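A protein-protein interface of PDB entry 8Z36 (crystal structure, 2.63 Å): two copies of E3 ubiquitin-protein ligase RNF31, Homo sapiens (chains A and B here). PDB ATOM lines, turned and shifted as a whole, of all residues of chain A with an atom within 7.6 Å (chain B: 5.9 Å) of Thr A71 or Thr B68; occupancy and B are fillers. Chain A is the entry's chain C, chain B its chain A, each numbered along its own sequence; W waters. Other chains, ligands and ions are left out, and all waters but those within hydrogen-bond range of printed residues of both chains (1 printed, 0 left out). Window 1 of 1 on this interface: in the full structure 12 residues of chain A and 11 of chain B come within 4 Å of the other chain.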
ATOM      1  N   ASN A  64     -13.732  -7.157  24.337  1.00  0.00           N
ATOM      2  CA  ASN A  64     -14.731  -8.108  24.812  1.00  0.00           C
ATOM      3  C   ASN A  64     -14.990  -7.974  26.310  1.00  0.00           C
ATOM      4  O   ASN A  64     -16.137  -7.788  26.728  1.00  0.00           O
ATOM      5  CB  ASN A  64     -14.297  -9.539  24.471  1.00  0.00           C
ATOM      6  CG  ASN A  64     -14.523  -9.882  23.012  1.00  0.00           C
ATOM      7  OD1 ASN A  64     -15.479  -9.415  22.394  1.00  0.00           O
ATOM      8  ND2 ASN A  64     -13.639 -10.700  22.453  1.00  0.00           N
ATOM      9  N   TYR A  65     -13.942  -8.066  27.132  1.00  0.00           N
ATOM     10  CA  TYR A  65     -14.167  -8.059  28.575  1.00  0.00           C
ATOM     11  C   TYR A  65     -14.486  -6.666  29.104  1.00  0.00           C
ATOM     12  O   TYR A  65     -15.137  -6.545  30.147  1.00  0.00           O
ATOM     13  CB  TYR A  65     -12.968  -8.666  29.315  1.00  0.00           C
ATOM     14  CG  TYR A  65     -11.634  -7.965  29.146  1.00  0.00           C
ATOM     15  CD1 TYR A  65     -11.370  -6.755  29.778  1.00  0.00           C
ATOM     16  CD2 TYR A  65     -10.619  -8.540  28.391  1.00  0.00           C
ATOM     17  CE1 TYR A  65     -10.148  -6.125  29.635  1.00  0.00           C
ATOM     18  CE2 TYR A  65      -9.394  -7.920  28.246  1.00  0.00           C
ATOM     19  CZ  TYR A  65      -9.164  -6.711  28.869  1.00  0.00           C
ATOM     20  OH  TYR A  65      -7.945  -6.088  28.728  1.00  0.00           O
ATOM     21  N   LEU A  66     -14.051  -5.610  28.411  1.00  0.00           N
ATOM     22  CA  LEU A  66     -14.473  -4.268  28.798  1.00  0.00           C
ATOM     23  C   LEU A  66     -15.963  -4.068  28.550  1.00  0.00           C
ATOM     24  O   LEU A  66     -16.625  -3.348  29.306  1.00  0.00           O
ATOM     25  CB  LEU A  66     -13.654  -3.215  28.048  1.00  0.00           C
ATOM     26  CG  LEU A  66     -12.177  -3.073  28.431  1.00  0.00           C
ATOM     27  CD1 LEU A  66     -11.581  -1.811  27.825  1.00  0.00           C
ATOM     28  CD2 LEU A  66     -11.992  -3.086  29.940  1.00  0.00           C
ATOM     29  N   ASN A  67     -16.503  -4.696  27.503  1.00  0.00           N
ATOM     30  CA  ASN A  67     -17.949  -4.692  27.301  1.00  0.00           C
ATOM     31  C   ASN A  67     -18.657  -5.505  28.377  1.00  0.00           C
ATOM     32  O   ASN A  67     -19.675  -5.066  28.926  1.00  0.00           O
ATOM     33  CB  ASN A  67     -18.285  -5.241  25.915  1.00  0.00           C
ATOM     34  CG  ASN A  67     -18.281  -4.172  24.842  1.00  0.00           C
ATOM     35  OD1 ASN A  67     -18.702  -4.415  23.713  1.00  0.00           O
ATOM     36  ND2 ASN A  67     -17.823  -2.979  25.193  1.00  0.00           N
ATOM     37  N   THR A  68     -18.138  -6.697  28.684  1.00  0.00           N
ATOM     38  CA  THR A  68     -18.737  -7.528  29.723  1.00  0.00           C
ATOM     39  C   THR A  68     -18.679  -6.839  31.081  1.00  0.00           C
ATOM     40  O   THR A  68     -19.626  -6.925  31.871  1.00  0.00           O
ATOM     41  CB  THR A  68     -18.030  -8.883  29.776  1.00  0.00           C
ATOM     42  OG1 THR A  68     -18.019  -9.467  28.468  1.00  0.00           O
ATOM     43  CG2 THR A  68     -18.741  -9.825  30.738  1.00  0.00           C
ATOM     44  N   LEU A  69     -17.576  -6.144  31.365  1.00  0.00           N
ATOM     45  CA  LEU A  69     -17.460  -5.421  32.628  1.00  0.00           C
ATOM     46  C   LEU A  69     -18.409  -4.230  32.672  1.00  0.00           C
ATOM     47  O   LEU A  69     -18.985  -3.928  33.725  1.00  0.00           O
ATOM     48  CB  LEU A  69     -16.015  -4.968  32.836  1.00  0.00           C
ATOM     49  CG  LEU A  69     -15.458  -5.005  34.261  1.00  0.00           C
ATOM     50  CD1 LEU A  69     -16.032  -6.176  35.043  1.00  0.00           C
ATOM     51  CD2 LEU A  69     -13.938  -5.068  34.235  1.00  0.00           C
ATOM     52  N   SER A  70     -18.589  -3.546  31.539  1.00  0.00           N
ATOM     53  CA  SER A  70     -19.453  -2.369  31.511  1.00  0.00           C
ATOM     54  C   SER A  70     -20.920  -2.751  31.665  1.00  0.00           C
ATOM     55  O   SER A  70     -21.674  -2.069  32.368  1.00  0.00           O
ATOM     56  CB  SER A  70     -19.238  -1.591  30.213  1.00  0.00           C
ATOM     57  OG  SER A  70     -18.078  -0.782  30.287  1.00  0.00           O
ATOM     58  N   THR A  71     -21.343  -3.836  31.012  1.00  0.00           N
ATOM     59  CA  THR A  71     -22.740  -4.251  31.106  1.00  0.00           C
ATOM     60  C   THR A  71     -23.072  -4.754  32.505  1.00  0.00           C
ATOM     61  O   THR A  71     -24.166  -4.493  33.020  1.00  0.00           O
ATOM     62  CB  THR A  71     -23.039  -5.325  30.060  1.00  0.00           C
ATOM     63  OG1 THR A  71     -22.622  -4.865  28.768  1.00  0.00           O
ATOM     64  CG2 THR A  71     -24.530  -5.632  30.020  1.00  0.00           C
ATOM     65  N   ALA A  72     -22.141  -5.471  33.138  1.00  0.00           N
ATOM     66  CA  ALA A  72     -22.372  -5.940  34.500  1.00  0.00           C
ATOM     67  C   ALA A  72     -22.494  -4.772  35.470  1.00  0.00           C
ATOM     68  O   ALA A  72     -23.318  -4.803  36.391  1.00  0.00           O
ATOM     69  CB  ALA A  72     -21.248  -6.881  34.930  1.00  0.00           C
ATOM     70  N   LEU A  73     -21.683  -3.729  35.277  1.00  0.00           N
ATOM     71  CA  LEU A  73     -21.767  -2.562  36.146  1.00  0.00           C
ATOM     72  C   LEU A  73     -23.015  -1.736  35.859  1.00  0.00           C
ATOM     73  O   LEU A  73     -23.537  -1.074  36.762  1.00  0.00           O
ATOM     74  CB  LEU A  73     -20.513  -1.705  35.998  1.00  0.00           C
ATOM     75  CG  LEU A  73     -19.260  -2.267  36.673  1.00  0.00           C
ATOM     76  CD1 LEU A  73     -18.009  -1.663  36.066  1.00  0.00           C
ATOM     77  CD2 LEU A  73     -19.304  -2.024  38.173  1.00  0.00           C
ATOM     78  N   ASN A  74     -23.502  -1.759  34.616  1.00  0.00           N
ATOM     79  CA  ASN A  74     -24.737  -1.049  34.297  1.00  0.00           C
ATOM     80  C   ASN A  74     -25.922  -1.656  35.036  1.00  0.00           C
ATOM     81  O   ASN A  74     -26.825  -0.934  35.478  1.00  0.00           O
ATOM     82  CB  ASN A  74     -24.978  -1.063  32.789  1.00  0.00           C
ATOM     83  CG  ASN A  74     -25.903   0.050  32.337  1.00  0.00           C
ATOM     84  OD1 ASN A  74     -25.862   1.160  32.867  1.00  0.00           O
ATOM     85  ND2 ASN A  74     -26.747  -0.244  31.354  1.00  0.00           N
ATOM     86  N   ILE A  75     -25.937  -2.979  35.183  1.00  0.00           N
ATOM     87  CA  ILE A  75     -27.001  -3.627  35.940  1.00  0.00           C
ATOM     88  C   ILE A  75     -26.793  -3.425  37.435  1.00  0.00           C
ATOM     89  O   ILE A  75     -27.756  -3.244  38.189  1.00  0.00           O
ATOM     90  CB  ILE A  75     -27.079  -5.118  35.568  1.00  0.00           C
ATOM     91  CG1 ILE A  75     -27.178  -5.265  34.048  1.00  0.00           C
ATOM     92  CG2 ILE A  75     -28.243  -5.798  36.286  1.00  0.00           C
ATOM     93  CD1 ILE A  75     -28.591  -5.351  33.527  1.00  0.00           C
ATOM     94  N   LEU A  76     -25.536  -3.448  37.887  1.00  0.00           N
ATOM     95  CA  LEU A  76     -25.254  -3.167  39.289  1.00  0.00           C
ATOM     96  C   LEU A  76     -25.607  -1.731  39.652  1.00  0.00           C
ATOM     97  O   LEU A  76     -26.025  -1.464  40.784  1.00  0.00           O
ATOM     98  CB  LEU A  76     -23.783  -3.449  39.597  1.00  0.00           C
ATOM     99  CG  LEU A  76     -23.390  -4.924  39.705  1.00  0.00           C
ATOM    100  CD1 LEU A  76     -21.876  -5.075  39.727  1.00  0.00           C
ATOM    101  CD2 LEU A  76     -24.016  -5.563  40.936  1.00  0.00           C
ATOM    102  N   GLU A  77     -25.446  -0.799  38.709  1.00  0.00           N
ATOM    103  CA  GLU A  77     -25.879   0.573  38.948  1.00  0.00           C
ATOM    104  C   GLU A  77     -27.395   0.667  39.046  1.00  0.00           C
ATOM    105  O   GLU A  77     -27.917   1.487  39.810  1.00  0.00           O
ATOM    106  CB  GLU A  77     -25.358   1.488  37.840  1.00  0.00           C
ATOM    107  CG  GLU A  77     -25.621   2.966  38.074  1.00  0.00           C
ATOM    108  CD  GLU A  77     -25.484   3.790  36.808  1.00  0.00           C
ATOM    109  OE1 GLU A  77     -24.672   3.413  35.938  1.00  0.00           O
ATOM    110  OE2 GLU A  77     -26.187   4.814  36.685  1.00  0.00           O
ATOM    111  N   VAL A 101     -31.363 -12.039  33.703  1.00  0.00           N
ATOM    112  CA  VAL A 101     -30.492 -10.893  33.478  1.00  0.00           C
ATOM    113  C   VAL A 101     -29.253 -10.974  34.366  1.00  0.00           C
ATOM    114  O   VAL A 101     -28.159 -10.570  33.954  1.00  0.00           O
ATOM    115  CB  VAL A 101     -31.281  -9.589  33.707  1.00  0.00           C
ATOM    116  CG1 VAL A 101     -30.346  -8.415  33.938  1.00  0.00           C
ATOM    117  CG2 VAL A 101     -32.203  -9.316  32.529  1.00  0.00           C
ATOM    118  N   ARG A 103     -27.554 -13.690  35.520  1.00  0.00           N
ATOM    119  CA  ARG A 103     -26.547 -14.658  35.089  1.00  0.00           C
ATOM    120  C   ARG A 103     -25.746 -14.136  33.903  1.00  0.00           C
ATOM    121  O   ARG A 103     -24.539 -14.385  33.805  1.00  0.00           O
ATOM    122  CB  ARG A 103     -27.203 -15.992  34.734  1.00  0.00           C
ATOM    123  CG  ARG A 103     -28.415 -16.354  35.573  1.00  0.00           C
ATOM    124  CD  ARG A 103     -29.053 -17.640  35.069  1.00  0.00           C
ATOM    125  NE  ARG A 103     -28.106 -18.748  35.056  1.00  0.00           N
ATOM    126  CZ  ARG A 103     -28.111 -19.728  34.163  1.00  0.00           C
ATOM    127  NH1 ARG A 103     -28.990 -19.758  33.176  1.00  0.00           N
ATOM    128  NH2 ARG A 103     -27.206 -20.698  34.260  1.00  0.00           N
ATOM    129  N   SER A 104     -26.397 -13.412  32.993  1.00  0.00           N
ATOM    130  CA  SER A 104     -25.737 -12.937  31.785  1.00  0.00           C
ATOM    131  C   SER A 104     -24.868 -11.708  32.016  1.00  0.00           C
ATOM    132  O   SER A 104     -24.057 -11.374  31.145  1.00  0.00           O
ATOM    133  CB  SER A 104     -26.778 -12.628  30.705  1.00  0.00           C
ATOM    134  OG  SER A 104     -27.413 -11.385  30.948  1.00  0.00           O
ATOM    135  N   THR A 105     -25.010 -11.028  33.156  1.00  0.00           N
ATOM    136  CA  THR A 105     -24.273  -9.792  33.406  1.00  0.00           C
ATOM    137  C   THR A 105     -23.463  -9.875  34.696  1.00  0.00           C
ATOM    138  O   THR A 105     -22.238  -9.994  34.633  1.00  0.00           O
ATOM    139  CB  THR A 105     -25.231  -8.598  33.432  1.00  0.00           C
ATOM    140  OG1 THR A 105     -26.225  -8.798  34.445  1.00  0.00           O
ATOM    141  CG2 THR A 105     -25.914  -8.427  32.080  1.00  0.00           C
ATOM    142  N   VAL A 106     -24.107  -9.819  35.862  1.00  0.00           N
ATOM    143  CA  VAL A 106     -23.370  -9.715  37.120  1.00  0.00           C
ATOM    144  C   VAL A 106     -22.619 -11.008  37.415  1.00  0.00           C
ATOM    145  O   VAL A 106     -21.410 -10.996  37.675  1.00  0.00           O
ATOM    146  CB  VAL A 106     -24.323  -9.341  38.268  1.00  0.00           C
ATOM    147  CG1 VAL A 106     -23.541  -9.122  39.555  1.00  0.00           C
ATOM    148  CG2 VAL A 106     -25.130  -8.104  37.907  1.00  0.00           C
ATOM    149  N   ALA A 108     -21.621 -13.175  35.494  1.00  0.00           N
ATOM    150  CA  ALA A 108     -20.599 -13.437  34.491  1.00  0.00           C
ATOM    151  C   ALA A 108     -19.303 -12.687  34.764  1.00  0.00           C
ATOM    152  O   ALA A 108     -18.367 -12.786  33.963  1.00  0.00           O
ATOM    153  CB  ALA A 108     -21.121 -13.073  33.099  1.00  0.00           C
ATOM    154  N   VAL A 109     -19.223 -11.947  35.867  1.00  0.00           N
ATOM    155  CA  VAL A 109     -18.052 -11.151  36.212  1.00  0.00           C
ATOM    156  C   VAL A 109     -17.562 -11.592  37.584  1.00  0.00           C
ATOM    157  O   VAL A 109     -18.355 -11.703  38.525  1.00  0.00           O
ATOM    158  CB  VAL A 109     -18.371  -9.643  36.196  1.00  0.00           C
ATOM    159  CG1 VAL A 109     -17.424  -8.877  37.109  1.00  0.00           C
ATOM    160  CG2 VAL A 109     -18.304  -9.106  34.774  1.00  0.00           C
ATOM    161  N   ARG A 154     -18.166   2.196  35.367  1.00  0.00           N
ATOM    162  CA  ARG A 154     -18.824   1.966  34.084  1.00  0.00           C
ATOM    163  C   ARG A 154     -18.465   3.054  33.081  1.00  0.00           C
ATOM    164  O   ARG A 154     -18.258   2.773  31.895  1.00  0.00           O
ATOM    165  CB  ARG A 154     -20.339   1.895  34.272  1.00  0.00           C
ATOM    166  CG  ARG A 154     -21.095   1.481  33.022  1.00  0.00           C
ATOM    167  CD  ARG A 154     -22.576   1.800  33.134  1.00  0.00           C
ATOM    168  NE  ARG A 154     -22.813   3.178  33.544  1.00  0.00           N
ATOM    169  CZ  ARG A 154     -23.641   4.011  32.926  1.00  0.00           C
ATOM    170  NH1 ARG A 154     -24.326   3.638  31.858  1.00  0.00           N
ATOM    171  NH2 ARG A 154     -23.782   5.249  33.390  1.00  0.00           N
ATOM    172  N   LEU A 157     -14.766   2.555  31.899  1.00  0.00           N
ATOM    173  CA  LEU A 157     -14.636   1.466  30.939  1.00  0.00           C
ATOM    174  C   LEU A 157     -15.293   1.811  29.609  1.00  0.00           C
ATOM    175  O   LEU A 157     -14.827   1.363  28.556  1.00  0.00           O
ATOM    176  CB  LEU A 157     -15.236   0.184  31.512  1.00  0.00           C
ATOM    177  CG  LEU A 157     -14.608  -0.344  32.803  1.00  0.00           C
ATOM    178  CD1 LEU A 157     -15.527  -1.351  33.465  1.00  0.00           C
ATOM    179  CD2 LEU A 157     -13.250  -0.963  32.531  1.00  0.00           C
ATOM    180  N   SER A 158     -16.367   2.606  29.635  1.00  0.00           N
ATOM    181  CA  SER A 158     -17.048   2.964  28.395  1.00  0.00           C
ATOM    182  C   SER A 158     -16.233   3.962  27.583  1.00  0.00           C
ATOM    183  O   SER A 158     -16.188   3.879  26.351  1.00  0.00           O
ATOM    184  CB  SER A 158     -18.436   3.527  28.703  1.00  0.00           C
ATOM    185  OG  SER A 158     -19.412   2.499  28.716  1.00  0.00           O
ATOM    186  N   ARG B  63     -30.211  -2.055  25.269  1.00  0.00           N
ATOM    187  CA  ARG B  63     -28.815  -1.639  25.280  1.00  0.00           C
ATOM    188  C   ARG B  63     -27.925  -2.591  26.067  1.00  0.00           C
ATOM    189  O   ARG B  63     -26.698  -2.514  25.938  1.00  0.00           O
ATOM    190  CB  ARG B  63     -28.693  -0.225  25.854  1.00  0.00           C
ATOM    191  N   ASN B  64     -28.505  -3.483  26.871  1.00  0.00           N
ATOM    192  CA  ASN B  64     -27.740  -4.432  27.669  1.00  0.00           C
ATOM    193  C   ASN B  64     -27.641  -5.800  26.999  1.00  0.00           C
ATOM    194  O   ASN B  64     -26.536  -6.283  26.736  1.00  0.00           O
ATOM    195  CB  ASN B  64     -28.362  -4.562  29.067  1.00  0.00           C
ATOM    196  CG  ASN B  64     -28.035  -3.380  29.962  1.00  0.00           C
ATOM    197  OD1 ASN B  64     -27.018  -2.712  29.782  1.00  0.00           O
ATOM    198  ND2 ASN B  64     -28.901  -3.118  30.935  1.00  0.00           N
ATOM    199  N   TYR B  65     -28.781  -6.436  26.711  1.00  0.00           N
ATOM    200  CA  TYR B  65     -28.732  -7.806  26.212  1.00  0.00           C
ATOM    201  C   TYR B  65     -28.263  -7.886  24.764  1.00  0.00           C
ATOM    202  O   TYR B  65     -27.741  -8.929  24.356  1.00  0.00           O
ATOM    203  CB  TYR B  65     -30.094  -8.497  26.385  1.00  0.00           C
ATOM    204  CG  TYR B  65     -31.255  -7.945  25.577  1.00  0.00           C
ATOM    205  CD1 TYR B  65     -31.347  -8.158  24.205  1.00  0.00           C
ATOM    206  CD2 TYR B  65     -32.286  -7.251  26.199  1.00  0.00           C
ATOM    207  CE1 TYR B  65     -32.412  -7.669  23.475  1.00  0.00           C
ATOM    208  CE2 TYR B  65     -33.357  -6.761  25.475  1.00  0.00           C
ATOM    209  CZ  TYR B  65     -33.414  -6.973  24.113  1.00  0.00           C
ATOM    210  OH  TYR B  65     -34.477  -6.486  23.388  1.00  0.00           O
ATOM    211  N   LEU B  66     -28.433  -6.820  23.978  1.00  0.00           N
ATOM    212  CA  LEU B  66     -27.865  -6.821  22.634  1.00  0.00           C
ATOM    213  C   LEU B  66     -26.344  -6.780  22.680  1.00  0.00           C
ATOM    214  O   LEU B  66     -25.682  -7.351  21.806  1.00  0.00           O
ATOM    215  CB  LEU B  66     -28.403  -5.642  21.822  1.00  0.00           C
ATOM    216  CG  LEU B  66     -29.892  -5.648  21.468  1.00  0.00           C
ATOM    217  CD1 LEU B  66     -30.265  -4.388  20.699  1.00  0.00           C
ATOM    218  CD2 LEU B  66     -30.265  -6.891  20.681  1.00  0.00           C
ATOM    219  N   ASN B  67     -25.776  -6.116  23.691  1.00  0.00           N
ATOM    220  CA  ASN B  67     -24.325  -6.103  23.843  1.00  0.00           C
ATOM    221  C   ASN B  67     -23.815  -7.437  24.372  1.00  0.00           C
ATOM    222  O   ASN B  67     -22.755  -7.916  23.950  1.00  0.00           O
ATOM    223  CB  ASN B  67     -23.907  -4.961  24.767  1.00  0.00           C
ATOM    224  CG  ASN B  67     -22.552  -4.387  24.404  1.00  0.00           C
ATOM    225  OD1 ASN B  67     -22.389  -3.775  23.348  1.00  0.00           O
ATOM    226  ND2 ASN B  67     -21.570  -4.584  25.277  1.00  0.00           N
ATOM    227  N   THR B  68     -24.553  -8.050  25.301  1.00  0.00           N
ATOM    228  CA  THR B  68     -24.179  -9.374  25.787  1.00  0.00           C
ATOM    229  C   THR B  68     -24.283 -10.413  24.677  1.00  0.00           C
ATOM    230  O   THR B  68     -23.434 -11.308  24.572  1.00  0.00           O
ATOM    231  CB  THR B  68     -25.059  -9.759  26.980  1.00  0.00           C
ATOM    232  OG1 THR B  68     -24.770  -8.893  28.084  1.00  0.00           O
ATOM    233  CG2 THR B  68     -24.810 -11.200  27.399  1.00  0.00           C
ATOM    234  N   LEU B  69     -25.307 -10.298  23.828  1.00  0.00           N
ATOM    235  CA  LEU B  69     -25.462 -11.231  22.717  1.00  0.00           C
ATOM    236  C   LEU B  69     -24.344 -11.069  21.694  1.00  0.00           C
ATOM    237  O   LEU B  69     -23.804 -12.062  21.194  1.00  0.00           O
ATOM    238  CB  LEU B  69     -26.827 -11.032  22.057  1.00  0.00           C
ATOM    239  CG  LEU B  69     -27.500 -12.257  21.436  1.00  0.00           C
ATOM    240  CD1 LEU B  69     -27.229 -13.505  22.259  1.00  0.00           C
ATOM    241  CD2 LEU B  69     -28.996 -12.024  21.287  1.00  0.00           C
ATOM    242  N   SER B  70     -23.982  -9.824  21.367  1.00  0.00           N
ATOM    243  CA  SER B  70     -22.933  -9.599  20.378  1.00  0.00           C
ATOM    244  C   SER B  70     -21.561  -9.984  20.914  1.00  0.00           C
ATOM    245  O   SER B  70     -20.699 -10.423  20.143  1.00  0.00           O
ATOM    246  CB  SER B  70     -22.934  -8.138  19.927  1.00  0.00           C
ATOM    247  OG  SER B  70     -23.285  -7.272  20.992  1.00  0.00           O
ATOM    248  N   THR B  71     -21.337  -9.825  22.220  1.00  0.00           N
ATOM    249  CA  THR B  71     -20.068 -10.251  22.803  1.00  0.00           C
ATOM    250  C   THR B  71     -19.928 -11.767  22.762  1.00  0.00           C
ATOM    251  O   THR B  71     -18.862 -12.288  22.414  1.00  0.00           O
ATOM    252  CB  THR B  71     -19.947  -9.740  24.239  1.00  0.00           C
ATOM    253  OG1 THR B  71     -20.126  -8.319  24.261  1.00  0.00           O
ATOM    254  CG2 THR B  71     -18.580 -10.084  24.814  1.00  0.00           C
ATOM    255  N   ALA B  72     -20.996 -12.490  23.109  1.00  0.00           N
ATOM    256  CA  ALA B  72     -20.957 -13.946  23.041  1.00  0.00           C
ATOM    257  C   ALA B  72     -20.790 -14.436  21.609  1.00  0.00           C
ATOM    258  O   ALA B  72     -20.127 -15.452  21.373  1.00  0.00           O
ATOM    259  CB  ALA B  72     -22.224 -14.535  23.660  1.00  0.00           C
ATOM    260  N   LEU B  73     -21.382 -13.730  20.642  1.00  0.00           N
ATOM    261  CA  LEU B  73     -21.207 -14.110  19.245  1.00  0.00           C
ATOM    262  C   LEU B  73     -19.799 -13.800  18.754  1.00  0.00           C
ATOM    263  O   LEU B  73     -19.275 -14.514  17.892  1.00  0.00           O
ATOM    264  CB  LEU B  73     -22.245 -13.405  18.374  1.00  0.00           C
ATOM    265  CG  LEU B  73     -23.652 -14.006  18.404  1.00  0.00           C
ATOM    266  CD1 LEU B  73     -24.646 -13.061  17.755  1.00  0.00           C
ATOM    267  CD2 LEU B  73     -23.676 -15.365  17.723  1.00  0.00           C
ATOM    268  N   THR B 105     -19.049 -15.150  28.624  1.00  0.00           N
ATOM    269  CA  THR B 105     -19.648 -14.633  27.395  1.00  0.00           C
ATOM    270  C   THR B 105     -20.604 -15.647  26.779  1.00  0.00           C
ATOM    271  O   THR B 105     -21.815 -15.418  26.784  1.00  0.00           O
ATOM    272  CB  THR B 105     -18.556 -14.227  26.402  1.00  0.00           C
ATOM    273  OG1 THR B 105     -17.844 -15.393  25.971  1.00  0.00           O
ATOM    274  CG2 THR B 105     -17.580 -13.251  27.046  1.00  0.00           C
ATOM    275  N   ALA B 108     -23.098 -17.451  29.134  1.00  0.00           N
ATOM    276  CA  ALA B 108     -24.082 -16.531  29.689  1.00  0.00           C
ATOM    277  C   ALA B 108     -25.265 -16.303  28.759  1.00  0.00           C
ATOM    278  O   ALA B 108     -26.171 -15.538  29.108  1.00  0.00           O
ATOM    279  CB  ALA B 108     -23.420 -15.190  30.021  1.00  0.00           C
ATOM    280  N   VAL B 109     -25.281 -16.945  27.594  1.00  0.00           N
ATOM    281  CA  VAL B 109     -26.326 -16.767  26.594  1.00  0.00           C
ATOM    282  C   VAL B 109     -27.028 -18.102  26.388  1.00  0.00           C
ATOM    283  O   VAL B 109     -26.372 -19.131  26.190  1.00  0.00           O
ATOM    284  CB  VAL B 109     -25.750 -16.235  25.268  1.00  0.00           C
ATOM    285  CG1 VAL B 109     -26.662 -16.587  24.103  1.00  0.00           C
ATOM    286  CG2 VAL B 109     -25.536 -14.731  25.351  1.00  0.00           C
HETATM  287  O   HOH W   1     -28.040  -9.171  29.086  1.00  0.00           O
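Hydrophobic or aromatic side chains of chain B within 4 Å of the printed part of chain A: Ala B108.
Of the 24 printed residues of chain A, 7 touch a printed residue of chain B.
Printed residues of chain A that touch a printed residue of chain B: Asn A64, Asn A67, Thr A68, Thr A71, Asn A74, Ile A75 and Ser A104.
Hydrophobic or aromatic side chains of chain A that line the printed part of chain B: Ile A75.
Asn A64 touches Thr B71, and with the chains exchanged Thr A71 touches Asn B64.
Asn A67 touches its own counterpart, Asn B67.
Asn A67 touches Thr B71, and with the chains exchanged Thr A71 touches Asn B67.
Thr A68 touches Thr B71, and with the chains exchanged Thr A71 touches Thr B68.
13 positions are printed for both chains.
Of the 11 pairs that touch across the chains among the printed residues, 7 have their exchanged pair printed and touching as well.
Thr A71 touches just these residues of chain B: Asn B64 (3.8 Å), Asn B67 (3.7 Å) and Thr B68 (3.8 Å).
Thr B68 touches just these residues of chain A: Thr A71 (3.8 Å) and Ser A104 (3.8 Å).
Printed residues of chain B within 4 Å of Asn A64: Thr B71 (3.9 Å).
Of the printed residues of chain A, Thr B71 touches Asn A64 (3.9 Å), Asn A67 (3.9 Å) and Thr A68 (3.7 Å).
Printed residues of chain B within 4 Å of Thr A68: Thr B71.
Of the printed residues of chain A, Asn B64 touches Thr A71, Asn A74 and Ile A75.
The nearest residue of chain B that does not touch Thr A71 is Tyr B65 (5.4 Å).
The nearest residue of chain A that does not touch Thr B68 is Thr A105 (4.2 Å).
The nearest printed residue of chain A that does not touch Ala B108 is Arg A103 (4.03 Å).
The side-chain amide oxygen (OD1) of Asn B64 is in hydrogen-bond range of the side-chain amide nitrogen (ND2) of Asn A74, 2.9 Å away.
The side-chain amide oxygen (OD1) of Asn A67 sits at hydrogen-bond distance from the side-chain amide nitrogen (ND2) of Asn B67 (3.3 Å).
CG2 of Thr B71 touches O of Asn A64, 3.9 Å away.
OG1 of Thr B71 touches CB of Asn A67 (3.9 Å).
CG2 of Thr B71 touches OG1 of Thr A68, at 3.7 Å.
Thr A71 touches Asn B64 (CG2 to OD1, 3.8 Å).
OG1 of Thr A71 touches ND2 of Asn B67 (3.7 Å).
Thr A71 touches Thr B68 (CG2 to OG1, 3.8 Å).
Asn B64 touches Ile A75.
Thr B68 touches Ser A104.
Ser A104 touches Ala B108 (CB to O, 3.4 Å).
Water W1 lies within hydrogen-bond range of OG of Ser A104 (3.0 Å) and OG1 of Thr B68 (3.4 Å).
The side-chain hydroxyl (OG1) of Thr A71 is in hydrogen-bond range of the backbone carbonyl oxygen (O) of Asn A67 (3.0 Å).
NH1 of Arg A154 is in hydrogen-bond range of OD1 of Asn A74, at 3.1 Å.
The backbone carbonyl oxygen of Asn A64 sits at hydrogen-bond distance from the side-chain hydroxyl of Thr A68, at 3.1 Å.
The side-chain hydroxyl (OG1) of Thr B68 sits at hydrogen-bond distance from the backbone carbonyl oxygen (O) of Asn B64.
The side-chain hydroxyl (OG) of Ser A104 lies within hydrogen-bond range of the backbone carbonyl oxygen (O) of Val A101, at 3.2 Å.
The backbone carbonyl oxygen (O) of Asn B67 sits at hydrogen-bond distance from the side-chain hydroxyl (OG) of Ser B70, at 3.1 Å.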
